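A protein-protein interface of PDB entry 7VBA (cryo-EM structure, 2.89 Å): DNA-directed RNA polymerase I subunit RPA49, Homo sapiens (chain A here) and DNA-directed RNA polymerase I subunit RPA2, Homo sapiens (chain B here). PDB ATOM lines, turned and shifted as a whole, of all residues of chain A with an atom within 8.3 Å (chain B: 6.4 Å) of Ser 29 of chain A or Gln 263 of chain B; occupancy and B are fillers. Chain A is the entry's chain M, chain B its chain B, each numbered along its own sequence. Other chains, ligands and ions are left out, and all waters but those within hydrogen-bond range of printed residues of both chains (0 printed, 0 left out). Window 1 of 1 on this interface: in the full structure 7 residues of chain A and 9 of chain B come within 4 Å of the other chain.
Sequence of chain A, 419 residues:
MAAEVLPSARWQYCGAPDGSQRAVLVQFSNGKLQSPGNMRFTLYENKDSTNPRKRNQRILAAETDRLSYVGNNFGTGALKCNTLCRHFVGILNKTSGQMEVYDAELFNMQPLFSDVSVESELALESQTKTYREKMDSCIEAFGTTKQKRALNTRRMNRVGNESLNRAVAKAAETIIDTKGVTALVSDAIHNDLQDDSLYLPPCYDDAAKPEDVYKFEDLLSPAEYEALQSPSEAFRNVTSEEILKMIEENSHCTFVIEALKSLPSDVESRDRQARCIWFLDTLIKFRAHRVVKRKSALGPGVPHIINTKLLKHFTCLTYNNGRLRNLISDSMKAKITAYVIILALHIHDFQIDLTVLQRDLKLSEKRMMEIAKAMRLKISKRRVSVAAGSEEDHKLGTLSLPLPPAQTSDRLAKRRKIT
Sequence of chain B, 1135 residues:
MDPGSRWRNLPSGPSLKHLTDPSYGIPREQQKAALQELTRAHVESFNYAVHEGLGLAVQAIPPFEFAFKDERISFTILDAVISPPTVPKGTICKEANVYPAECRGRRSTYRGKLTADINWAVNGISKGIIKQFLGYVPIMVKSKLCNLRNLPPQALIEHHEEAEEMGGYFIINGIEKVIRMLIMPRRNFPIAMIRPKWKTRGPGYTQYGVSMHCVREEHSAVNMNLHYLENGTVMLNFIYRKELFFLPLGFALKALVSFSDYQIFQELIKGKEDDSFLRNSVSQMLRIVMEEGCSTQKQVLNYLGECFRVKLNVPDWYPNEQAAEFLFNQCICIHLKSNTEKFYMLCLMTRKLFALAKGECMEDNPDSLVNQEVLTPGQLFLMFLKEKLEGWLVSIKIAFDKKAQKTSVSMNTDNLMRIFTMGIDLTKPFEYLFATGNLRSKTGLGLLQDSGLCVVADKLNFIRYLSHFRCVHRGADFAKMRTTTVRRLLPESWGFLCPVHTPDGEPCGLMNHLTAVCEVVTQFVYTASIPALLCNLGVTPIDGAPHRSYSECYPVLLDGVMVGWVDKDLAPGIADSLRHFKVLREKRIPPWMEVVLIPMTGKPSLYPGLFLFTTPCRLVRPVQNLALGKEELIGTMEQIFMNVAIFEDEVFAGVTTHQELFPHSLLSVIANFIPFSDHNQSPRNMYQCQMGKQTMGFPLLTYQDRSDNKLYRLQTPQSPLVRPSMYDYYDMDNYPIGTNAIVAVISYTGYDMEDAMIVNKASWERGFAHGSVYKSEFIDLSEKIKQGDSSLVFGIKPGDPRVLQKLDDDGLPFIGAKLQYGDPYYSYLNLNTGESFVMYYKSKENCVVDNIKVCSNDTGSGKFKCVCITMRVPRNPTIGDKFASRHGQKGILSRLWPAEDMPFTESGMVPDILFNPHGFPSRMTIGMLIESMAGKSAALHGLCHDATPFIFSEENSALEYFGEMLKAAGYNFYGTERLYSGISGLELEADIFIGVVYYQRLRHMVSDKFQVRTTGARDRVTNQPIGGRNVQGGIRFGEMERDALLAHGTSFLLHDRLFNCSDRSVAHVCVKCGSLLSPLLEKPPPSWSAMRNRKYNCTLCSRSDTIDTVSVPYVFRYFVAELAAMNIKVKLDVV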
ATOM      1  N   VAL A  26      -0.919 -21.453 -27.544  1.00  0.00           N
ATOM      2  CA  VAL A  26      -1.782 -21.341 -26.372  1.00  0.00           C
ATOM      3  C   VAL A  26      -1.066 -20.551 -25.278  1.00  0.00           C
ATOM      4  O   VAL A  26       0.160 -20.617 -25.156  1.00  0.00           O
ATOM      5  CB  VAL A  26      -2.200 -22.730 -25.839  1.00  0.00           C
ATOM      6  CG1 VAL A  26      -3.018 -23.485 -26.885  1.00  0.00           C
ATOM      7  CG2 VAL A  26      -0.969 -23.538 -25.432  1.00  0.00           C
ATOM      8  N   GLN A  27      -1.844 -19.744 -24.637  1.00  0.00           N
ATOM      9  CA  GLN A  27      -1.419 -18.992 -23.462  1.00  0.00           C
ATOM     10  C   GLN A  27      -2.410 -19.159 -22.313  1.00  0.00           C
ATOM     11  O   GLN A  27      -3.613 -18.965 -22.492  1.00  0.00           O
ATOM     12  CB  GLN A  27      -1.256 -17.509 -23.803  1.00  0.00           C
ATOM     13  CG  GLN A  27      -0.698 -16.672 -22.661  1.00  0.00           C
ATOM     14  CD  GLN A  27      -0.523 -15.212 -23.032  1.00  0.00           C
ATOM     15  OE1 GLN A  27      -1.314 -14.654 -23.798  1.00  0.00           O
ATOM     16  NE2 GLN A  27       0.516 -14.583 -22.494  1.00  0.00           N
ATOM     17  N   PHE A  28      -1.927 -19.488 -21.138  1.00  0.00           N
ATOM     18  CA  PHE A  28      -2.775 -19.719 -19.975  1.00  0.00           C
ATOM     19  C   PHE A  28      -2.892 -18.458 -19.129  1.00  0.00           C
ATOM     20  O   PHE A  28      -1.885 -17.821 -18.814  1.00  0.00           O
ATOM     21  CB  PHE A  28      -2.226 -20.872 -19.129  1.00  0.00           C
ATOM     22  CG  PHE A  28      -2.329 -22.217 -19.794  1.00  0.00           C
ATOM     23  CD1 PHE A  28      -1.335 -22.651 -20.664  1.00  0.00           C
ATOM     24  CD2 PHE A  28      -3.414 -23.048 -19.550  1.00  0.00           C
ATOM     25  CE1 PHE A  28      -1.424 -23.895 -21.282  1.00  0.00           C
ATOM     26  CE2 PHE A  28      -3.510 -24.295 -20.165  1.00  0.00           C
ATOM     27  CZ  PHE A  28      -2.511 -24.715 -21.030  1.00  0.00           C
ATOM     28  N   SER A  29      -4.042 -18.020 -18.787  1.00  0.00           N
ATOM     29  CA  SER A  29      -4.298 -16.787 -18.051  1.00  0.00           C
ATOM     30  C   SER A  29      -3.729 -16.857 -16.639  1.00  0.00           C
ATOM     31  O   SER A  29      -3.421 -15.826 -16.036  1.00  0.00           O
ATOM     32  CB  SER A  29      -5.799 -16.500 -17.991  1.00  0.00           C
ATOM     33  OG  SER A  29      -6.495 -17.583 -17.399  1.00  0.00           O
ATOM     34  N   ASN A  30      -3.554 -18.057 -16.060  1.00  0.00           N
ATOM     35  CA  ASN A  30      -3.129 -18.184 -14.670  1.00  0.00           C
ATOM     36  C   ASN A  30      -1.670 -18.618 -14.566  1.00  0.00           C
ATOM     37  O   ASN A  30      -1.262 -19.208 -13.565  1.00  0.00           O
ATOM     38  CB  ASN A  30      -4.030 -19.167 -13.920  1.00  0.00           C
ATOM     39  CG  ASN A  30      -5.463 -18.685 -13.818  1.00  0.00           C
ATOM     40  OD1 ASN A  30      -5.722 -17.481 -13.751  1.00  0.00           O
ATOM     41  ND2 ASN A  30      -6.405 -19.621 -13.804  1.00  0.00           N
ATOM     42  N   GLY A  31      -0.940 -18.398 -15.625  1.00  0.00           N
ATOM     43  CA  GLY A  31       0.469 -18.748 -15.550  1.00  0.00           C
ATOM     44  C   GLY A  31       0.846 -19.901 -16.459  1.00  0.00           C
ATOM     45  O   GLY A  31       0.308 -20.032 -17.560  1.00  0.00           O
ATOM     46  N   LYS A  32       1.978 -20.611 -16.062  1.00  0.00           N
ATOM     47  CA  LYS A  32       2.554 -21.701 -16.846  1.00  0.00           C
ATOM     48  C   LYS A  32       2.126 -23.058 -16.297  1.00  0.00           C
ATOM     49  O   LYS A  32       1.905 -23.205 -15.092  1.00  0.00           O
ATOM     50  CB  LYS A  32       4.079 -21.600 -16.866  1.00  0.00           C
ATOM     51  CG  LYS A  32       4.754 -22.602 -17.792  1.00  0.00           C
ATOM     52  CD  LYS A  32       6.266 -22.422 -17.803  1.00  0.00           C
ATOM     53  CE  LYS A  32       6.947 -23.463 -18.681  1.00  0.00           C
ATOM     54  NZ  LYS A  32       8.433 -23.309 -18.671  1.00  0.00           N
ATOM     55  N   LEU A  33       2.250 -24.091 -17.131  1.00  0.00           N
ATOM     56  CA  LEU A  33       2.085 -25.473 -16.638  1.00  0.00           C
ATOM     57  C   LEU A  33       3.511 -26.000 -16.570  1.00  0.00           C
ATOM     58  O   LEU A  33       4.160 -26.012 -17.628  1.00  0.00           O
ATOM     59  CB  LEU A  33       1.324 -26.241 -17.703  1.00  0.00           C
ATOM     60  CG  LEU A  33       0.529 -25.329 -18.615  1.00  0.00           C
ATOM     61  CD1 LEU A  33       0.350 -25.994 -19.954  1.00  0.00           C
ATOM     62  CD2 LEU A  33      -0.796 -24.968 -17.965  1.00  0.00           C
ATOM     63  N   TYR A  69      -9.563 -26.279 -19.392  1.00  0.00           N
ATOM     64  CA  TYR A  69      -9.303 -24.945 -19.921  1.00  0.00           C
ATOM     65  C   TYR A  69      -9.935 -24.773 -21.298  1.00  0.00           C
ATOM     66  O   TYR A  69      -9.978 -25.717 -22.089  1.00  0.00           O
ATOM     67  CB  TYR A  69      -7.797 -24.680 -20.001  1.00  0.00           C
ATOM     68  CG  TYR A  69      -7.107 -24.694 -18.659  1.00  0.00           C
ATOM     69  CD1 TYR A  69      -6.730 -25.893 -18.064  1.00  0.00           C
ATOM     70  CD2 TYR A  69      -6.828 -23.507 -17.985  1.00  0.00           C
ATOM     71  CE1 TYR A  69      -6.092 -25.911 -16.827  1.00  0.00           C
ATOM     72  CE2 TYR A  69      -6.189 -23.514 -16.749  1.00  0.00           C
ATOM     73  CZ  TYR A  69      -5.827 -24.719 -16.179  1.00  0.00           C
ATOM     74  OH  TYR A  69      -5.195 -24.732 -14.956  1.00  0.00           O
ATOM     75  N   VAL A  70     -10.446 -23.537 -21.469  1.00  0.00           N
ATOM     76  CA  VAL A  70     -11.058 -23.286 -22.769  1.00  0.00           C
ATOM     77  C   VAL A  70     -10.596 -21.934 -23.306  1.00  0.00           C
ATOM     78  O   VAL A  70     -10.440 -20.977 -22.545  1.00  0.00           O
ATOM     79  CB  VAL A  70     -12.601 -23.328 -22.688  1.00  0.00           C
ATOM     80  CG1 VAL A  70     -13.224 -22.954 -24.032  1.00  0.00           C
ATOM     81  CG2 VAL A  70     -13.075 -24.710 -22.242  1.00  0.00           C
ATOM     82  N   LEU A  79      -9.367 -12.028 -27.612  1.00  0.00           N
ATOM     83  CA  LEU A  79      -8.762 -10.784 -27.119  1.00  0.00           C
ATOM     84  C   LEU A  79      -8.274  -9.942 -28.301  1.00  0.00           C
ATOM     85  O   LEU A  79      -8.342 -10.435 -29.435  1.00  0.00           O
ATOM     86  CB  LEU A  79      -7.709 -11.186 -26.092  1.00  0.00           C
ATOM     87  CG  LEU A  79      -8.278 -11.522 -24.711  1.00  0.00           C
ATOM     88  CD1 LEU A  79      -7.201 -11.471 -23.637  1.00  0.00           C
ATOM     89  CD2 LEU A  79      -9.410 -10.570 -24.355  1.00  0.00           C
ATOM     90  N   PHE A 107      -4.502 -18.795 -28.727  1.00  0.00           N
ATOM     91  CA  PHE A 107      -5.642 -19.040 -27.851  1.00  0.00           C
ATOM     92  C   PHE A 107      -5.287 -18.728 -26.401  1.00  0.00           C
ATOM     93  O   PHE A 107      -4.312 -19.261 -25.867  1.00  0.00           O
ATOM     94  CB  PHE A 107      -6.115 -20.490 -27.974  1.00  0.00           C
ATOM     95  CG  PHE A 107      -6.765 -20.806 -29.296  1.00  0.00           C
ATOM     96  CD1 PHE A 107      -5.993 -21.144 -30.398  1.00  0.00           C
ATOM     97  CD2 PHE A 107      -8.146 -20.766 -29.434  1.00  0.00           C
ATOM     98  CE1 PHE A 107      -6.588 -21.437 -31.622  1.00  0.00           C
ATOM     99  CE2 PHE A 107      -8.750 -21.058 -30.655  1.00  0.00           C
ATOM    100  CZ  PHE A 107      -7.966 -21.393 -31.748  1.00  0.00           C
ATOM    101  N   ASN A 108      -6.036 -17.864 -25.786  1.00  0.00           N
ATOM    102  CA  ASN A 108      -5.905 -17.626 -24.353  1.00  0.00           C
ATOM    103  C   ASN A 108      -6.768 -18.590 -23.544  1.00  0.00           C
ATOM    104  O   ASN A 108      -7.998 -18.534 -23.607  1.00  0.00           O
ATOM    105  CB  ASN A 108      -6.268 -16.178 -24.015  1.00  0.00           C
ATOM    106  CG  ASN A 108      -5.280 -15.180 -24.587  1.00  0.00           C
ATOM    107  OD1 ASN A 108      -4.071 -15.415 -24.588  1.00  0.00           O
ATOM    108  ND2 ASN A 108      -5.791 -14.058 -25.079  1.00  0.00           N
ATOM    109  N   MET A 109      -6.074 -19.425 -22.824  1.00  0.00           N
ATOM    110  CA  MET A 109      -6.763 -20.507 -22.126  1.00  0.00           C
ATOM    111  C   MET A 109      -7.251 -20.048 -20.756  1.00  0.00           C
ATOM    112  O   MET A 109      -6.473 -19.512 -19.962  1.00  0.00           O
ATOM    113  CB  MET A 109      -5.845 -21.720 -21.974  1.00  0.00           C
ATOM    114  CG  MET A 109      -5.291 -22.239 -23.292  1.00  0.00           C
ATOM    115  SD  MET A 109      -6.611 -22.801 -24.435  1.00  0.00           S
ATOM    116  CE  MET A 109      -7.161 -24.302 -23.579  1.00  0.00           C
ATOM    117  N   GLN A 110      -8.430 -20.660 -20.401  1.00  0.00           N
ATOM    118  CA  GLN A 110      -9.155 -20.357 -19.123  1.00  0.00           C
ATOM    119  C   GLN A 110      -9.907 -21.568 -18.508  1.00  0.00           C
ATOM    120  O   GLN A 110     -10.523 -22.288 -19.265  1.00  0.00           O
ATOM    121  CB  GLN A 110     -10.333 -19.451 -19.470  1.00  0.00           C
ATOM    122  CG  GLN A 110     -10.049 -17.970 -19.317  1.00  0.00           C
ATOM    123  CD  GLN A 110     -10.754 -17.426 -18.101  1.00  0.00           C
ATOM    124  OE1 GLN A 110     -11.857 -17.848 -17.765  1.00  0.00           O
ATOM    125  NE2 GLN A 110     -10.114 -16.481 -17.434  1.00  0.00           N
ATOM    126  N   PRO A 111     -10.046 -21.730 -17.161  1.00  0.00           N
ATOM    127  CA  PRO A 111     -10.750 -22.874 -16.456  1.00  0.00           C
ATOM    128  C   PRO A 111     -12.255 -23.173 -16.625  1.00  0.00           C
ATOM    129  O   PRO A 111     -13.006 -22.218 -16.684  1.00  0.00           O
ATOM    130  CB  PRO A 111     -10.594 -22.548 -14.969  1.00  0.00           C
ATOM    131  CG  PRO A 111      -9.352 -21.706 -14.926  1.00  0.00           C
ATOM    132  CD  PRO A 111      -9.465 -20.832 -16.157  1.00  0.00           C
ATOM    133  N   SER B 258     -14.783 -11.911 -16.698  1.00  0.00           N
ATOM    134  CA  SER B 258     -14.878 -13.335 -16.298  1.00  0.00           C
ATOM    135  C   SER B 258     -13.484 -13.945 -16.362  1.00  0.00           C
ATOM    136  O   SER B 258     -13.253 -14.793 -17.225  1.00  0.00           O
ATOM    137  CB  SER B 258     -15.800 -14.078 -17.193  1.00  0.00           C
ATOM    138  OG  SER B 258     -15.428 -13.892 -18.548  1.00  0.00           O
ATOM    139  N   PHE B 259     -12.590 -13.487 -15.495  1.00  0.00           N
ATOM    140  CA  PHE B 259     -11.198 -13.990 -15.465  1.00  0.00           C
ATOM    141  C   PHE B 259     -10.975 -14.585 -14.084  1.00  0.00           C
ATOM    142  O   PHE B 259     -11.753 -14.279 -13.175  1.00  0.00           O
ATOM    143  CB  PHE B 259     -10.186 -12.851 -15.547  1.00  0.00           C
ATOM    144  CG  PHE B 259      -9.865 -12.249 -16.888  1.00  0.00           C
ATOM    145  CD1 PHE B 259     -10.332 -12.805 -18.063  1.00  0.00           C
ATOM    146  CD2 PHE B 259      -9.053 -11.128 -16.961  1.00  0.00           C
ATOM    147  CE1 PHE B 259     -10.006 -12.236 -19.285  1.00  0.00           C
ATOM    148  CE2 PHE B 259      -8.727 -10.562 -18.181  1.00  0.00           C
ATOM    149  CZ  PHE B 259      -9.207 -11.118 -19.342  1.00  0.00           C
ATOM    150  N   SER B 260      -9.897 -15.334 -13.924  1.00  0.00           N
ATOM    151  CA  SER B 260      -9.585 -16.014 -12.658  1.00  0.00           C
ATOM    152  C   SER B 260      -9.121 -14.949 -11.686  1.00  0.00           C
ATOM    153  O   SER B 260      -8.842 -13.852 -12.148  1.00  0.00           O
ATOM    154  CB  SER B 260      -8.505 -16.938 -12.952  1.00  0.00           C
ATOM    155  OG  SER B 260      -8.045 -16.720 -14.272  1.00  0.00           O
ATOM    156  N   ASP B 261      -9.048 -15.236 -10.394  1.00  0.00           N
ATOM    157  CA  ASP B 261      -8.502 -14.220  -9.469  1.00  0.00           C
ATOM    158  C   ASP B 261      -6.993 -14.089  -9.632  1.00  0.00           C
ATOM    159  O   ASP B 261      -6.499 -13.059  -9.248  1.00  0.00           O
ATOM    160  CB  ASP B 261      -8.906 -14.515  -8.038  1.00  0.00           C
ATOM    161  CG  ASP B 261     -10.186 -13.816  -7.630  1.00  0.00           C
ATOM    162  OD1 ASP B 261     -10.534 -12.829  -8.291  1.00  0.00           O
ATOM    163  OD2 ASP B 261     -10.821 -14.265  -6.653  1.00  0.00           O
ATOM    164  N   TYR B 262      -6.288 -15.073 -10.174  1.00  0.00           N
ATOM    165  CA  TYR B 262      -4.845 -14.907 -10.415  1.00  0.00           C
ATOM    166  C   TYR B 262      -4.616 -14.002 -11.595  1.00  0.00           C
ATOM    167  O   TYR B 262      -3.728 -13.187 -11.506  1.00  0.00           O
ATOM    168  CB  TYR B 262      -4.163 -16.181 -10.868  1.00  0.00           C
ATOM    169  CG  TYR B 262      -2.661 -16.102 -10.928  1.00  0.00           C
ATOM    170  CD1 TYR B 262      -1.921 -15.565  -9.894  1.00  0.00           C
ATOM    171  CD2 TYR B 262      -1.974 -16.578 -12.023  1.00  0.00           C
ATOM    172  CE1 TYR B 262      -0.539 -15.505  -9.949  1.00  0.00           C
ATOM    173  CE2 TYR B 262      -0.596 -16.531 -12.100  1.00  0.00           C
ATOM    174  CZ  TYR B 262       0.126 -15.992 -11.058  1.00  0.00           C
ATOM    175  OH  TYR B 262       1.485 -15.950 -11.148  1.00  0.00           O
ATOM    176  N   GLN B 263      -5.374 -14.141 -12.669  1.00  0.00           N
ATOM    177  CA  GLN B 263      -5.230 -13.213 -13.821  1.00  0.00           C
ATOM    178  C   GLN B 263      -5.602 -11.775 -13.447  1.00  0.00           C
ATOM    179  O   GLN B 263      -4.871 -10.885 -13.843  1.00  0.00           O
ATOM    180  CB  GLN B 263      -5.938 -13.745 -15.054  1.00  0.00           C
ATOM    181  CG  GLN B 263      -5.464 -13.110 -16.344  1.00  0.00           C
ATOM    182  CD  GLN B 263      -6.451 -13.421 -17.436  1.00  0.00           C
ATOM    183  OE1 GLN B 263      -7.463 -14.074 -17.203  1.00  0.00           O
ATOM    184  NE2 GLN B 263      -6.155 -12.971 -18.642  1.00  0.00           N
ATOM    185  N   ILE B 264      -6.660 -11.542 -12.688  1.00  0.00           N
ATOM    186  CA  ILE B 264      -6.929 -10.159 -12.210  1.00  0.00           C
ATOM    187  C   ILE B 264      -5.696  -9.671 -11.440  1.00  0.00           C
ATOM    188  O   ILE B 264      -5.291  -8.547 -11.663  1.00  0.00           O
ATOM    189  CB  ILE B 264      -8.198 -10.129 -11.351  1.00  0.00           C
ATOM    190  CG1 ILE B 264      -9.448 -10.384 -12.189  1.00  0.00           C
ATOM    191  CG2 ILE B 264      -8.304  -8.829 -10.576  1.00  0.00           C
ATOM    192  CD1 ILE B 264     -10.702 -10.509 -11.370  1.00  0.00           C
ATOM    193  N   PHE B 265      -5.082 -10.498 -10.600  1.00  0.00           N
ATOM    194  CA  PHE B 265      -3.913 -10.142  -9.754  1.00  0.00           C
ATOM    195  C   PHE B 265      -2.693  -9.896 -10.606  1.00  0.00           C
ATOM    196  O   PHE B 265      -2.028  -8.914 -10.410  1.00  0.00           O
ATOM    197  CB  PHE B 265      -3.608 -11.338  -8.859  1.00  0.00           C
ATOM    198  CG  PHE B 265      -2.273 -11.438  -8.170  1.00  0.00           C
ATOM    199  CD1 PHE B 265      -2.112 -10.982  -6.878  1.00  0.00           C
ATOM    200  CD2 PHE B 265      -1.211 -12.088  -8.770  1.00  0.00           C
ATOM    201  CE1 PHE B 265      -0.898 -11.102  -6.229  1.00  0.00           C
ATOM    202  CE2 PHE B 265       0.005 -12.209  -8.122  1.00  0.00           C
ATOM    203  CZ  PHE B 265       0.155 -11.718  -6.852  1.00  0.00           C
ATOM    204  N   GLN B 266      -2.446 -10.751 -11.570  1.00  0.00           N
ATOM    205  CA  GLN B 266      -1.232 -10.624 -12.383  1.00  0.00           C
ATOM    206  C   GLN B 266      -1.299  -9.253 -13.060  1.00  0.00           C
ATOM    207  O   GLN B 266      -0.227  -8.738 -13.360  1.00  0.00           O
ATOM    208  CB  GLN B 266      -1.074 -11.903 -13.202  1.00  0.00           C
ATOM    209  CG  GLN B 266      -0.434 -11.718 -14.562  1.00  0.00           C
ATOM    210  CD  GLN B 266      -0.436 -13.047 -15.269  1.00  0.00           C
ATOM    211  OE1 GLN B 266      -0.389 -14.095 -14.634  1.00  0.00           O
ATOM    212  NE2 GLN B 266      -0.503 -13.011 -16.589  1.00  0.00           N
ATOM    213  N   GLU B 267      -2.491  -8.720 -13.365  1.00  0.00           N
ATOM    214  CA  GLU B 267      -2.691  -7.351 -13.932  1.00  0.00           C
ATOM    215  C   GLU B 267      -2.426  -6.206 -12.946  1.00  0.00           C
ATOM    216  O   GLU B 267      -1.877  -5.206 -13.385  1.00  0.00           O
ATOM    217  CB  GLU B 267      -4.058  -7.195 -14.594  1.00  0.00           C
ATOM    218  CG  GLU B 267      -4.093  -7.637 -16.045  1.00  0.00           C
ATOM    219  CD  GLU B 267      -4.365  -9.111 -16.303  1.00  0.00           C
ATOM    220  OE1 GLU B 267      -3.414  -9.913 -16.246  1.00  0.00           O
ATOM    221  OE2 GLU B 267      -5.531  -9.456 -16.571  1.00  0.00           O
ATOM    222  N   LEU B 268      -2.825  -6.285 -11.683  1.00  0.00           N
ATOM    223  CA  LEU B 268      -2.649  -5.120 -10.776  1.00  0.00           C
ATOM    224  C   LEU B 268      -1.222  -5.071 -10.219  1.00  0.00           C
ATOM    225  O   LEU B 268      -0.948  -4.157  -9.457  1.00  0.00           O
ATOM    226  CB  LEU B 268      -3.661  -5.163  -9.634  1.00  0.00           C
ATOM    227  CG  LEU B 268      -5.139  -5.209  -9.985  1.00  0.00           C
ATOM    228  CD1 LEU B 268      -5.855  -6.175  -9.061  1.00  0.00           C
ATOM    229  CD2 LEU B 268      -5.738  -3.834  -9.817  1.00  0.00           C
ATOM    230  N   LYS B 270       1.493  -5.462 -12.326  1.00  0.00           N
ATOM    231  CA  LYS B 270       2.256  -5.593 -13.588  1.00  0.00           C
ATOM    232  C   LYS B 270       3.655  -5.006 -13.448  1.00  0.00           C
ATOM    233  O   LYS B 270       4.603  -5.730 -13.736  1.00  0.00           O
ATOM    234  CB  LYS B 270       1.463  -5.018 -14.763  1.00  0.00           C
ATOM    235  CG  LYS B 270       1.428  -5.844 -16.034  1.00  0.00           C
ATOM    236  CD  LYS B 270       0.307  -6.845 -16.080  1.00  0.00           C
ATOM    237  CE  LYS B 270      -0.031  -7.278 -17.489  1.00  0.00           C
ATOM    238  NZ  LYS B 270      -0.903  -8.474 -17.509  1.00  0.00           N
ATOM    239  N   PHE B 343     -12.207  -2.759 -17.352  1.00  0.00           N
ATOM    240  CA  PHE B 343     -11.334  -3.449 -16.374  1.00  0.00           C
ATOM    241  C   PHE B 343      -9.904  -2.943 -16.484  1.00  0.00           C
ATOM    242  O   PHE B 343      -9.369  -2.536 -15.474  1.00  0.00           O
ATOM    243  CB  PHE B 343     -11.318  -4.951 -16.642  1.00  0.00           C
ATOM    244  CG  PHE B 343     -10.296  -5.760 -15.891  1.00  0.00           C
ATOM    245  CD1 PHE B 343     -10.451  -6.028 -14.546  1.00  0.00           C
ATOM    246  CD2 PHE B 343      -9.203  -6.296 -16.543  1.00  0.00           C
ATOM    247  CE1 PHE B 343      -9.517  -6.786 -13.864  1.00  0.00           C
ATOM    248  CE2 PHE B 343      -8.269  -7.054 -15.862  1.00  0.00           C
ATOM    249  CZ  PHE B 343      -8.429  -7.298 -14.524  1.00  0.00           C
ATOM    250  N   TYR B 344      -9.338  -2.879 -17.674  1.00  0.00           N
ATOM    251  CA  TYR B 344      -7.931  -2.477 -17.818  1.00  0.00           C
ATOM    252  C   TYR B 344      -7.756  -1.027 -17.359  1.00  0.00           C
ATOM    253  O   TYR B 344      -6.675  -0.697 -16.898  1.00  0.00           O
ATOM    254  CB  TYR B 344      -7.455  -2.809 -19.220  1.00  0.00           C
ATOM    255  CG  TYR B 344      -7.175  -4.260 -19.502  1.00  0.00           C
ATOM    256  CD1 TYR B 344      -6.100  -4.907 -18.924  1.00  0.00           C
ATOM    257  CD2 TYR B 344      -7.952  -4.973 -20.392  1.00  0.00           C
ATOM    258  CE1 TYR B 344      -5.821  -6.234 -19.200  1.00  0.00           C
ATOM    259  CE2 TYR B 344      -7.688  -6.299 -20.682  1.00  0.00           C
ATOM    260  CZ  TYR B 344      -6.618  -6.932 -20.086  1.00  0.00           C
ATOM    261  OH  TYR B 344      -6.350  -8.237 -20.371  1.00  0.00           O
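Printed residues of chain B within 4 Å of Ser 29 of chain A: Ser 260, Gln 263 and Gln 266. Val 70 of chain A touches none of the printed residues of chain B. Of the printed residues of chain A, Ser 260 of chain B touches Ser 29, Asn 30 and Gln 110. Of the printed residues of chain A, Tyr 262 of chain B touches Asn 30. Of the printed residues of chain A, Gln 263 of chain B touches Ser 29 (3.0 Å), Asn 30 (3.5 Å) and Gln 110 (3.6 Å). Printed residues of chain A within 4 Å of Gln 266 of chain B: Ser 29 (3.8 Å). The nearest residue of chain A that does not touch Gln 263 of chain B is Leu 79 of chain A (5.3 Å). The nearest printed residue of chain B that does not touch Asn 30 of chain A is Gln 266 of chain B (4.7 Å).
N of Ser 29 of chain A sits at hydrogen-bond distance from O of Met 109 of chain A (3.1 Å). N of Val 70 of chain A sits at hydrogen-bond distance from O of Gln 110 of chain A (2.5 Å).
Printed residues of chain B that touch a printed residue of chain A: Ser 258, Phe 259, Ser 260, Tyr 262, Gln 263 and Gln 266. Hydrophobic or aromatic side chains of chain B within 4 Å of the printed part of chain A: Phe 259 and Tyr 262. Among the printed residues, 10 pairs touch across the chains.
OG of Ser 260 of chain B touches OG of Ser 29 of chain A, at 3.6 Å. Gln 263 of chain B touches Ser 29 of chain A (OE1 to CB, 3.0 Å). Ser 29 of chain A touches Gln 266 of chain B (O to OE1, 3.8 Å). Asn 30 of chain A touches Tyr 262 of chain B. Gln 263 of chain B touches Asn 30 of chain A. Gln 110 of chain A touches Phe 259 of chain B (NE2 to CA, 3.4 Å). Gln 110 of chain A touches Ser 260 of chain B. Gln 110 of chain A touches Gln 263 of chain B.
The backbone carbonyl oxygen (O) of Ser 258 of chain B sits close to the side-chain amide oxygen (OE1) of Gln 110 of chain A, at 3.4 Å. OG of Ser 260 of chain B is in hydrogen-bond range of OD1 of Asn 30 of chain A, at 2.5 Å.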
